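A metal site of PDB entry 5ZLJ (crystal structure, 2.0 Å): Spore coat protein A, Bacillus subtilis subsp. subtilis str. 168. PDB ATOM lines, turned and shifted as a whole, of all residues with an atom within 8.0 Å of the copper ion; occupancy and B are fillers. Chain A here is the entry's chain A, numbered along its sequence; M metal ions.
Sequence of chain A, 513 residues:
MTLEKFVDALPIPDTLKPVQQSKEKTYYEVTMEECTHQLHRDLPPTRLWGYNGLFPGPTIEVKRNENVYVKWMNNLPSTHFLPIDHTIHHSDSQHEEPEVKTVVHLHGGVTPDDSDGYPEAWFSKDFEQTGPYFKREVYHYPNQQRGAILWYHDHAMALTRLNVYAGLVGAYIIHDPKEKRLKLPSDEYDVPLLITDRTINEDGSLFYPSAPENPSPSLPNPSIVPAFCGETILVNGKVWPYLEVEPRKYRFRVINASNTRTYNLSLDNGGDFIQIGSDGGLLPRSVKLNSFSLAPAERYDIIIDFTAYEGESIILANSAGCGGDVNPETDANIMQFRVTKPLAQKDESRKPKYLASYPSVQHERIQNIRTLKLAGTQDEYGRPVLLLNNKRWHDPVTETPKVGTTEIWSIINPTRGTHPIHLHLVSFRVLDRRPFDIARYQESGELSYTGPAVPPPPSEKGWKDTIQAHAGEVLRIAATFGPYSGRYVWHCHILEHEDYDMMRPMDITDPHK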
ATOM      1  N   PRO A 226       6.402  21.343 -26.360  1.00  0.00           N
ATOM      2  CA  PRO A 226       5.061  21.230 -26.960  1.00  0.00           C
ATOM      3  C   PRO A 226       4.220  20.119 -26.386  1.00  0.00           C
ATOM      4  O   PRO A 226       3.074  19.961 -26.800  1.00  0.00           O
ATOM      5  CB  PRO A 226       5.348  20.932 -28.433  1.00  0.00           C
ATOM      6  CG  PRO A 226       6.699  20.287 -28.429  1.00  0.00           C
ATOM      7  CD  PRO A 226       7.461  20.853 -27.276  1.00  0.00           C
ATOM      8  N   LEU A 374      -7.174  23.994 -36.984  1.00  0.00           N
ATOM      9  CA  LEU A 374      -6.133  23.796 -36.015  1.00  0.00           C
ATOM     10  C   LEU A 374      -4.807  23.764 -36.759  1.00  0.00           C
ATOM     11  O   LEU A 374      -4.581  22.919 -37.593  1.00  0.00           O
ATOM     12  CB  LEU A 374      -6.328  22.473 -35.275  1.00  0.00           C
ATOM     13  CG  LEU A 374      -7.734  22.266 -34.666  1.00  0.00           C
ATOM     14  CD1 LEU A 374      -7.766  20.966 -33.844  1.00  0.00           C
ATOM     15  CD2 LEU A 374      -8.177  23.458 -33.848  1.00  0.00           C
ATOM     16  N   ALA A 375      -3.932  24.693 -36.430  1.00  0.00           N
ATOM     17  CA  ALA A 375      -2.685  24.842 -37.171  1.00  0.00           C
ATOM     18  C   ALA A 375      -1.573  25.402 -36.269  1.00  0.00           C
ATOM     19  O   ALA A 375      -1.515  25.105 -35.085  1.00  0.00           O
ATOM     20  CB  ALA A 375      -2.919  25.736 -38.395  1.00  0.00           C
ATOM     21  N   LEU A 386       1.452  26.619 -31.718  1.00  0.00           N
ATOM     22  CA  LEU A 386       0.184  26.047 -32.124  1.00  0.00           C
ATOM     23  C   LEU A 386      -0.915  27.117 -32.063  1.00  0.00           C
ATOM     24  O   LEU A 386      -1.036  27.824 -31.054  1.00  0.00           O
ATOM     25  CB  LEU A 386      -0.153  24.850 -31.248  1.00  0.00           C
ATOM     26  CG  LEU A 386       0.872  23.745 -31.503  1.00  0.00           C
ATOM     27  CD1 LEU A 386       1.780  23.460 -30.320  1.00  0.00           C
ATOM     28  CD2 LEU A 386       0.171  22.513 -32.018  1.00  0.00           C
ATOM     29  N   LEU A 387      -1.714  27.218 -33.119  1.00  0.00           N
ATOM     30  CA  LEU A 387      -2.681  28.300 -33.303  1.00  0.00           C
ATOM     31  C   LEU A 387      -4.039  27.804 -33.732  1.00  0.00           C
ATOM     32  O   LEU A 387      -4.172  26.826 -34.464  1.00  0.00           O
ATOM     33  CB  LEU A 387      -2.168  29.285 -34.368  1.00  0.00           C
ATOM     34  CG  LEU A 387      -0.814  29.928 -34.127  1.00  0.00           C
ATOM     35  CD1 LEU A 387      -0.470  30.878 -35.291  1.00  0.00           C
ATOM     36  CD2 LEU A 387      -0.783  30.645 -32.809  1.00  0.00           C
ATOM     37  N   LEU A 388      -5.073  28.530 -33.278  1.00  0.00           N
ATOM     38  CA  LEU A 388      -6.425  28.257 -33.704  1.00  0.00           C
ATOM     39  C   LEU A 388      -6.743  29.271 -34.842  1.00  0.00           C
ATOM     40  O   LEU A 388      -6.631  30.495 -34.653  1.00  0.00           O
ATOM     41  CB  LEU A 388      -7.380  28.447 -32.540  1.00  0.00           C
ATOM     42  CG  LEU A 388      -7.134  27.553 -31.309  1.00  0.00           C
ATOM     43  CD1 LEU A 388      -7.999  28.032 -30.179  1.00  0.00           C
ATOM     44  CD2 LEU A 388      -7.409  26.110 -31.629  1.00  0.00           C
ATOM     45  N   ASN A 413      -8.839  19.522 -38.416  1.00  0.00           N
ATOM     46  CA  ASN A 413      -7.554  19.186 -37.858  1.00  0.00           C
ATOM     47  C   ASN A 413      -6.640  18.529 -38.886  1.00  0.00           C
ATOM     48  O   ASN A 413      -6.702  17.299 -39.048  1.00  0.00           O
ATOM     49  CB  ASN A 413      -7.695  18.200 -36.681  1.00  0.00           C
ATOM     50  CG  ASN A 413      -6.359  17.960 -36.003  1.00  0.00           C
ATOM     51  OD1 ASN A 413      -5.330  18.500 -36.406  1.00  0.00           O
ATOM     52  ND2 ASN A 413      -6.374  17.139 -34.972  1.00  0.00           N
ATOM     53  N   THR A 415      -3.360  18.485 -38.482  1.00  0.00           N
ATOM     54  CA  THR A 415      -2.087  18.214 -37.802  1.00  0.00           C
ATOM     55  C   THR A 415      -1.952  16.726 -37.624  1.00  0.00           C
ATOM     56  O   THR A 415      -2.848  15.976 -37.968  1.00  0.00           O
ATOM     57  CB  THR A 415      -1.955  18.922 -36.399  1.00  0.00           C
ATOM     58  OG1 THR A 415      -2.811  18.275 -35.414  1.00  0.00           O
ATOM     59  CG2 THR A 415      -2.253  20.437 -36.496  1.00  0.00           C
ATOM     60  N   GLY A 417      -1.734  15.124 -34.695  1.00  0.00           N
ATOM     61  CA  GLY A 417      -2.236  14.556 -33.432  1.00  0.00           C
ATOM     62  C   GLY A 417      -3.623  15.034 -33.076  1.00  0.00           C
ATOM     63  O   GLY A 417      -4.178  15.933 -33.730  1.00  0.00           O
ATOM     64  N   THR A 418      -4.192  14.416 -32.050  1.00  0.00           N
ATOM     65  CA  THR A 418      -5.465  14.818 -31.498  1.00  0.00           C
ATOM     66  C   THR A 418      -5.340  16.057 -30.616  1.00  0.00           C
ATOM     67  O   THR A 418      -4.345  16.207 -29.920  1.00  0.00           O
ATOM     68  CB  THR A 418      -6.058  13.652 -30.670  1.00  0.00           C
ATOM     69  OG1 THR A 418      -6.324  12.563 -31.546  1.00  0.00           O
ATOM     70  CG2 THR A 418      -7.369  14.017 -30.005  1.00  0.00           C
ATOM     71  N   HIS A 419      -6.312  16.989 -30.706  1.00  0.00           N
ATOM     72  CA  HIS A 419      -6.381  18.127 -29.801  1.00  0.00           C
ATOM     73  C   HIS A 419      -7.697  18.099 -29.054  1.00  0.00           C
ATOM     74  O   HIS A 419      -8.744  18.056 -29.693  1.00  0.00           O
ATOM     75  CB  HIS A 419      -6.246  19.446 -30.564  1.00  0.00           C
ATOM     76  CG  HIS A 419      -4.976  19.551 -31.328  1.00  0.00           C
ATOM     77  ND1 HIS A 419      -3.824  19.982 -30.750  1.00  0.00           N
ATOM     78  CD2 HIS A 419      -4.659  19.218 -32.606  1.00  0.00           C
ATOM     79  CE1 HIS A 419      -2.839  19.957 -31.638  1.00  0.00           C
ATOM     80  NE2 HIS A 419      -3.318  19.459 -32.764  1.00  0.00           N
ATOM     81  N   PRO A 420      -7.665  18.113 -27.710  1.00  0.00           N
ATOM     82  CA  PRO A 420      -8.915  18.177 -26.964  1.00  0.00           C
ATOM     83  C   PRO A 420      -9.378  19.625 -26.850  1.00  0.00           C
ATOM     84  O   PRO A 420      -8.786  20.399 -26.113  1.00  0.00           O
ATOM     85  CB  PRO A 420      -8.551  17.605 -25.590  1.00  0.00           C
ATOM     86  CG  PRO A 420      -7.113  17.968 -25.425  1.00  0.00           C
ATOM     87  CD  PRO A 420      -6.498  18.018 -26.816  1.00  0.00           C
ATOM     88  N   ILE A 421     -10.386  19.998 -27.630  1.00  0.00           N
ATOM     89  CA  ILE A 421     -10.875  21.365 -27.688  1.00  0.00           C
ATOM     90  C   ILE A 421     -11.947  21.610 -26.630  1.00  0.00           C
ATOM     91  O   ILE A 421     -12.914  20.862 -26.539  1.00  0.00           O
ATOM     92  CB  ILE A 421     -11.421  21.679 -29.086  1.00  0.00           C
ATOM     93  CG1 ILE A 421     -10.354  21.381 -30.157  1.00  0.00           C
ATOM     94  CG2 ILE A 421     -11.943  23.138 -29.124  1.00  0.00           C
ATOM     95  CD1 ILE A 421      -9.077  22.174 -30.005  1.00  0.00           C
ATOM     96  N   ALA A 469     -10.595  16.274 -31.101  1.00  0.00           N
ATOM     97  CA  ALA A 469     -10.555  16.552 -32.536  1.00  0.00           C
ATOM     98  C   ALA A 469      -9.365  15.780 -33.056  1.00  0.00           C
ATOM     99  O   ALA A 469      -8.213  16.192 -32.868  1.00  0.00           O
ATOM    100  CB  ALA A 469     -10.409  18.045 -32.785  1.00  0.00           C
ATOM    101  N   HIS A 491     -10.180  26.884 -26.477  1.00  0.00           N
ATOM    102  CA  HIS A 491      -8.788  26.500 -26.562  1.00  0.00           C
ATOM    103  C   HIS A 491      -8.556  25.001 -26.573  1.00  0.00           C
ATOM    104  O   HIS A 491      -9.445  24.187 -26.203  1.00  0.00           O
ATOM    105  CB  HIS A 491      -7.992  27.117 -25.406  1.00  0.00           C
ATOM    106  CG  HIS A 491      -8.417  26.644 -24.043  1.00  0.00           C
ATOM    107  ND1 HIS A 491      -7.719  25.693 -23.332  1.00  0.00           N
ATOM    108  CD2 HIS A 491      -9.430  27.051 -23.237  1.00  0.00           C
ATOM    109  CE1 HIS A 491      -8.308  25.494 -22.174  1.00  0.00           C
ATOM    110  NE2 HIS A 491      -9.330  26.317 -22.085  1.00  0.00           N
ATOM    111  N   CYS A 492      -7.351  24.636 -26.981  1.00  0.00           N
ATOM    112  CA  CYS A 492      -6.870  23.273 -26.815  1.00  0.00           C
ATOM    113  C   CYS A 492      -6.507  23.096 -25.343  1.00  0.00           C
ATOM    114  O   CYS A 492      -5.919  23.996 -24.727  1.00  0.00           O
ATOM    115  CB  CYS A 492      -5.659  23.000 -27.702  1.00  0.00           C
ATOM    116  SG  CYS A 492      -4.988  21.366 -27.383  1.00  0.00           S
ATOM    117  N   HIS A 493      -6.861  21.940 -24.784  1.00  0.00           N
ATOM    118  CA  HIS A 493      -6.594  21.683 -23.377  1.00  0.00           C
ATOM    119  C   HIS A 493      -5.366  20.856 -23.119  1.00  0.00           C
ATOM    120  O   HIS A 493      -5.143  20.373 -21.996  1.00  0.00           O
ATOM    121  CB  HIS A 493      -7.831  21.088 -22.667  1.00  0.00           C
ATOM    122  CG  HIS A 493      -7.987  21.620 -21.265  1.00  0.00           C
ATOM    123  ND1 HIS A 493      -7.143  21.244 -20.241  1.00  0.00           N
ATOM    124  CD2 HIS A 493      -8.875  22.490 -20.728  1.00  0.00           C
ATOM    125  CE1 HIS A 493      -7.495  21.890 -19.129  1.00  0.00           C
ATOM    126  NE2 HIS A 493      -8.541  22.647 -19.405  1.00  0.00           N
ATOM    127  N   ILE A 494      -4.531  20.653 -24.136  1.00  0.00           N
ATOM    128  CA  ILE A 494      -3.165  20.271 -23.874  1.00  0.00           C
ATOM    129  C   ILE A 494      -2.470  21.563 -23.449  1.00  0.00           C
ATOM    130  O   ILE A 494      -2.383  22.535 -24.236  1.00  0.00           O
ATOM    131  CB  ILE A 494      -2.483  19.636 -25.105  1.00  0.00           C
ATOM    132  CG1 ILE A 494      -3.162  18.299 -25.413  1.00  0.00           C
ATOM    133  CG2 ILE A 494      -0.986  19.483 -24.882  1.00  0.00           C
ATOM    134  CD1 ILE A 494      -2.818  17.696 -26.750  1.00  0.00           C
ATOM    135  N   LEU A 495      -2.026  21.601 -22.200  1.00  0.00           N
ATOM    136  CA  LEU A 495      -1.662  22.881 -21.591  1.00  0.00           C
ATOM    137  C   LEU A 495      -0.420  23.472 -22.249  1.00  0.00           C
ATOM    138  O   LEU A 495      -0.333  24.691 -22.433  1.00  0.00           O
ATOM    139  CB  LEU A 495      -1.487  22.765 -20.087  1.00  0.00           C
ATOM    140  CG  LEU A 495      -2.716  22.243 -19.358  1.00  0.00           C
ATOM    141  CD1 LEU A 495      -2.480  22.262 -17.838  1.00  0.00           C
ATOM    142  CD2 LEU A 495      -3.977  23.027 -19.716  1.00  0.00           C
ATOM    143  N   GLU A 496       0.496  22.598 -22.668  1.00  0.00           N
ATOM    144  CA  GLU A 496       1.679  22.995 -23.430  1.00  0.00           C
ATOM    145  C   GLU A 496       1.326  23.681 -24.780  1.00  0.00           C
ATOM    146  O   GLU A 496       2.080  24.527 -25.280  1.00  0.00           O
ATOM    147  CB  GLU A 496       2.595  21.791 -23.658  1.00  0.00           C
ATOM    148  CG  GLU A 496       3.392  21.316 -22.448  1.00  0.00           C
ATOM    149  CD  GLU A 496       2.568  20.730 -21.301  1.00  0.00           C
ATOM    150  OE1 GLU A 496       1.453  20.198 -21.560  1.00  0.00           O
ATOM    151  OE2 GLU A 496       3.050  20.830 -20.136  1.00  0.00           O
ATOM    152  N   HIS A 497       0.183  23.300 -25.367  1.00  0.00           N
ATOM    153  CA  HIS A 497      -0.313  23.961 -26.571  1.00  0.00           C
ATOM    154  C   HIS A 497      -1.010  25.253 -26.224  1.00  0.00           C
ATOM    155  O   HIS A 497      -0.818  26.283 -26.884  1.00  0.00           O
ATOM    156  CB  HIS A 497      -1.318  23.064 -27.275  1.00  0.00           C
ATOM    157  CG  HIS A 497      -0.709  21.809 -27.800  1.00  0.00           C
ATOM    158  ND1 HIS A 497      -1.429  20.893 -28.530  1.00  0.00           N
ATOM    159  CD2 HIS A 497       0.553  21.343 -27.726  1.00  0.00           C
ATOM    160  CE1 HIS A 497      -0.616  19.886 -28.866  1.00  0.00           C
ATOM    161  NE2 HIS A 497       0.574  20.134 -28.383  1.00  0.00           N
ATOM    162  N   GLU A 498      -1.887  25.172 -25.220  1.00  0.00           N
ATOM    163  CA  GLU A 498      -2.684  26.307 -24.746  1.00  0.00           C
ATOM    164  C   GLU A 498      -1.813  27.541 -24.487  1.00  0.00           C
ATOM    165  O   GLU A 498      -2.201  28.658 -24.864  1.00  0.00           O
ATOM    166  CB  GLU A 498      -3.426  25.910 -23.460  1.00  0.00           C
ATOM    167  CG  GLU A 498      -4.171  27.040 -22.791  1.00  0.00           C
ATOM    168  CD  GLU A 498      -4.964  26.551 -21.592  1.00  0.00           C
ATOM    169  OE1 GLU A 498      -5.310  25.365 -21.530  1.00  0.00           O
ATOM    170  OE2 GLU A 498      -5.294  27.365 -20.752  1.00  0.00           O
ATOM    171  N   MET A 502      -2.422  28.165 -28.361  1.00  0.00           N
ATOM    172  CA  MET A 502      -3.615  27.544 -28.923  1.00  0.00           C
ATOM    173  C   MET A 502      -4.864  27.850 -28.091  1.00  0.00           C
ATOM    174  O   MET A 502      -5.557  26.964 -27.595  1.00  0.00           O
ATOM    175  CB  MET A 502      -3.360  26.072 -29.125  1.00  0.00           C
ATOM    176  CG  MET A 502      -4.245  25.392 -30.128  1.00  0.00           C
ATOM    177  SD  MET A 502      -3.666  23.725 -30.484  1.00  0.00           S
ATOM    178  CE  MET A 502      -4.748  23.247 -31.788  1.00  0.00           C
HETATM  179 CU    CU M   1      -3.482  20.968 -28.911  1.00  0.00          CU
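The side-chain sulfur of Cys 492 lies close to the backbone NH of Ile 494 (3.4 Å). O of Pro 226 is in hydrogen-bond range of NE2 of His 497, at 3.0 Å. ND1 of His 419 lies close to SD of Met 502 (3.8 Å). OG1 of Thr 415 sits at hydrogen-bond distance from NE2 of His 419, at 2.9 Å. The backbone NH of Cys 492 lies within hydrogen-bond range of the backbone carbonyl oxygen of Met 502, 3.0 Å away. O of Leu 386 sits at hydrogen-bond distance from N of Met 502 (3.0 Å). The backbone carbonyl oxygen of His 497 sits at hydrogen-bond distance from the backbone NH of Met 502, at 2.9 Å. O of His 419 sits at hydrogen-bond distance from N of Ala 469 (2.9 Å).
Residues that only touch the copper ion: Met 502 and Ile 494. Within 4 Å of the copper ion: His 419, Cys 492, Ile 494, His 497 and Met 502. Along chain A the residues within 4 Å of the copper ion span positions 419 to 502. The nearest printed residue that does not touch the copper ion is Pro 420 (4.7 Å).
A ring nitrogen (ND1) of His 497 is bound to the copper ion. A ring nitrogen (ND1) of His 419 binds the copper ion (2.1 Å). SG of Cys 492 binds the copper ion (2.2 Å).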
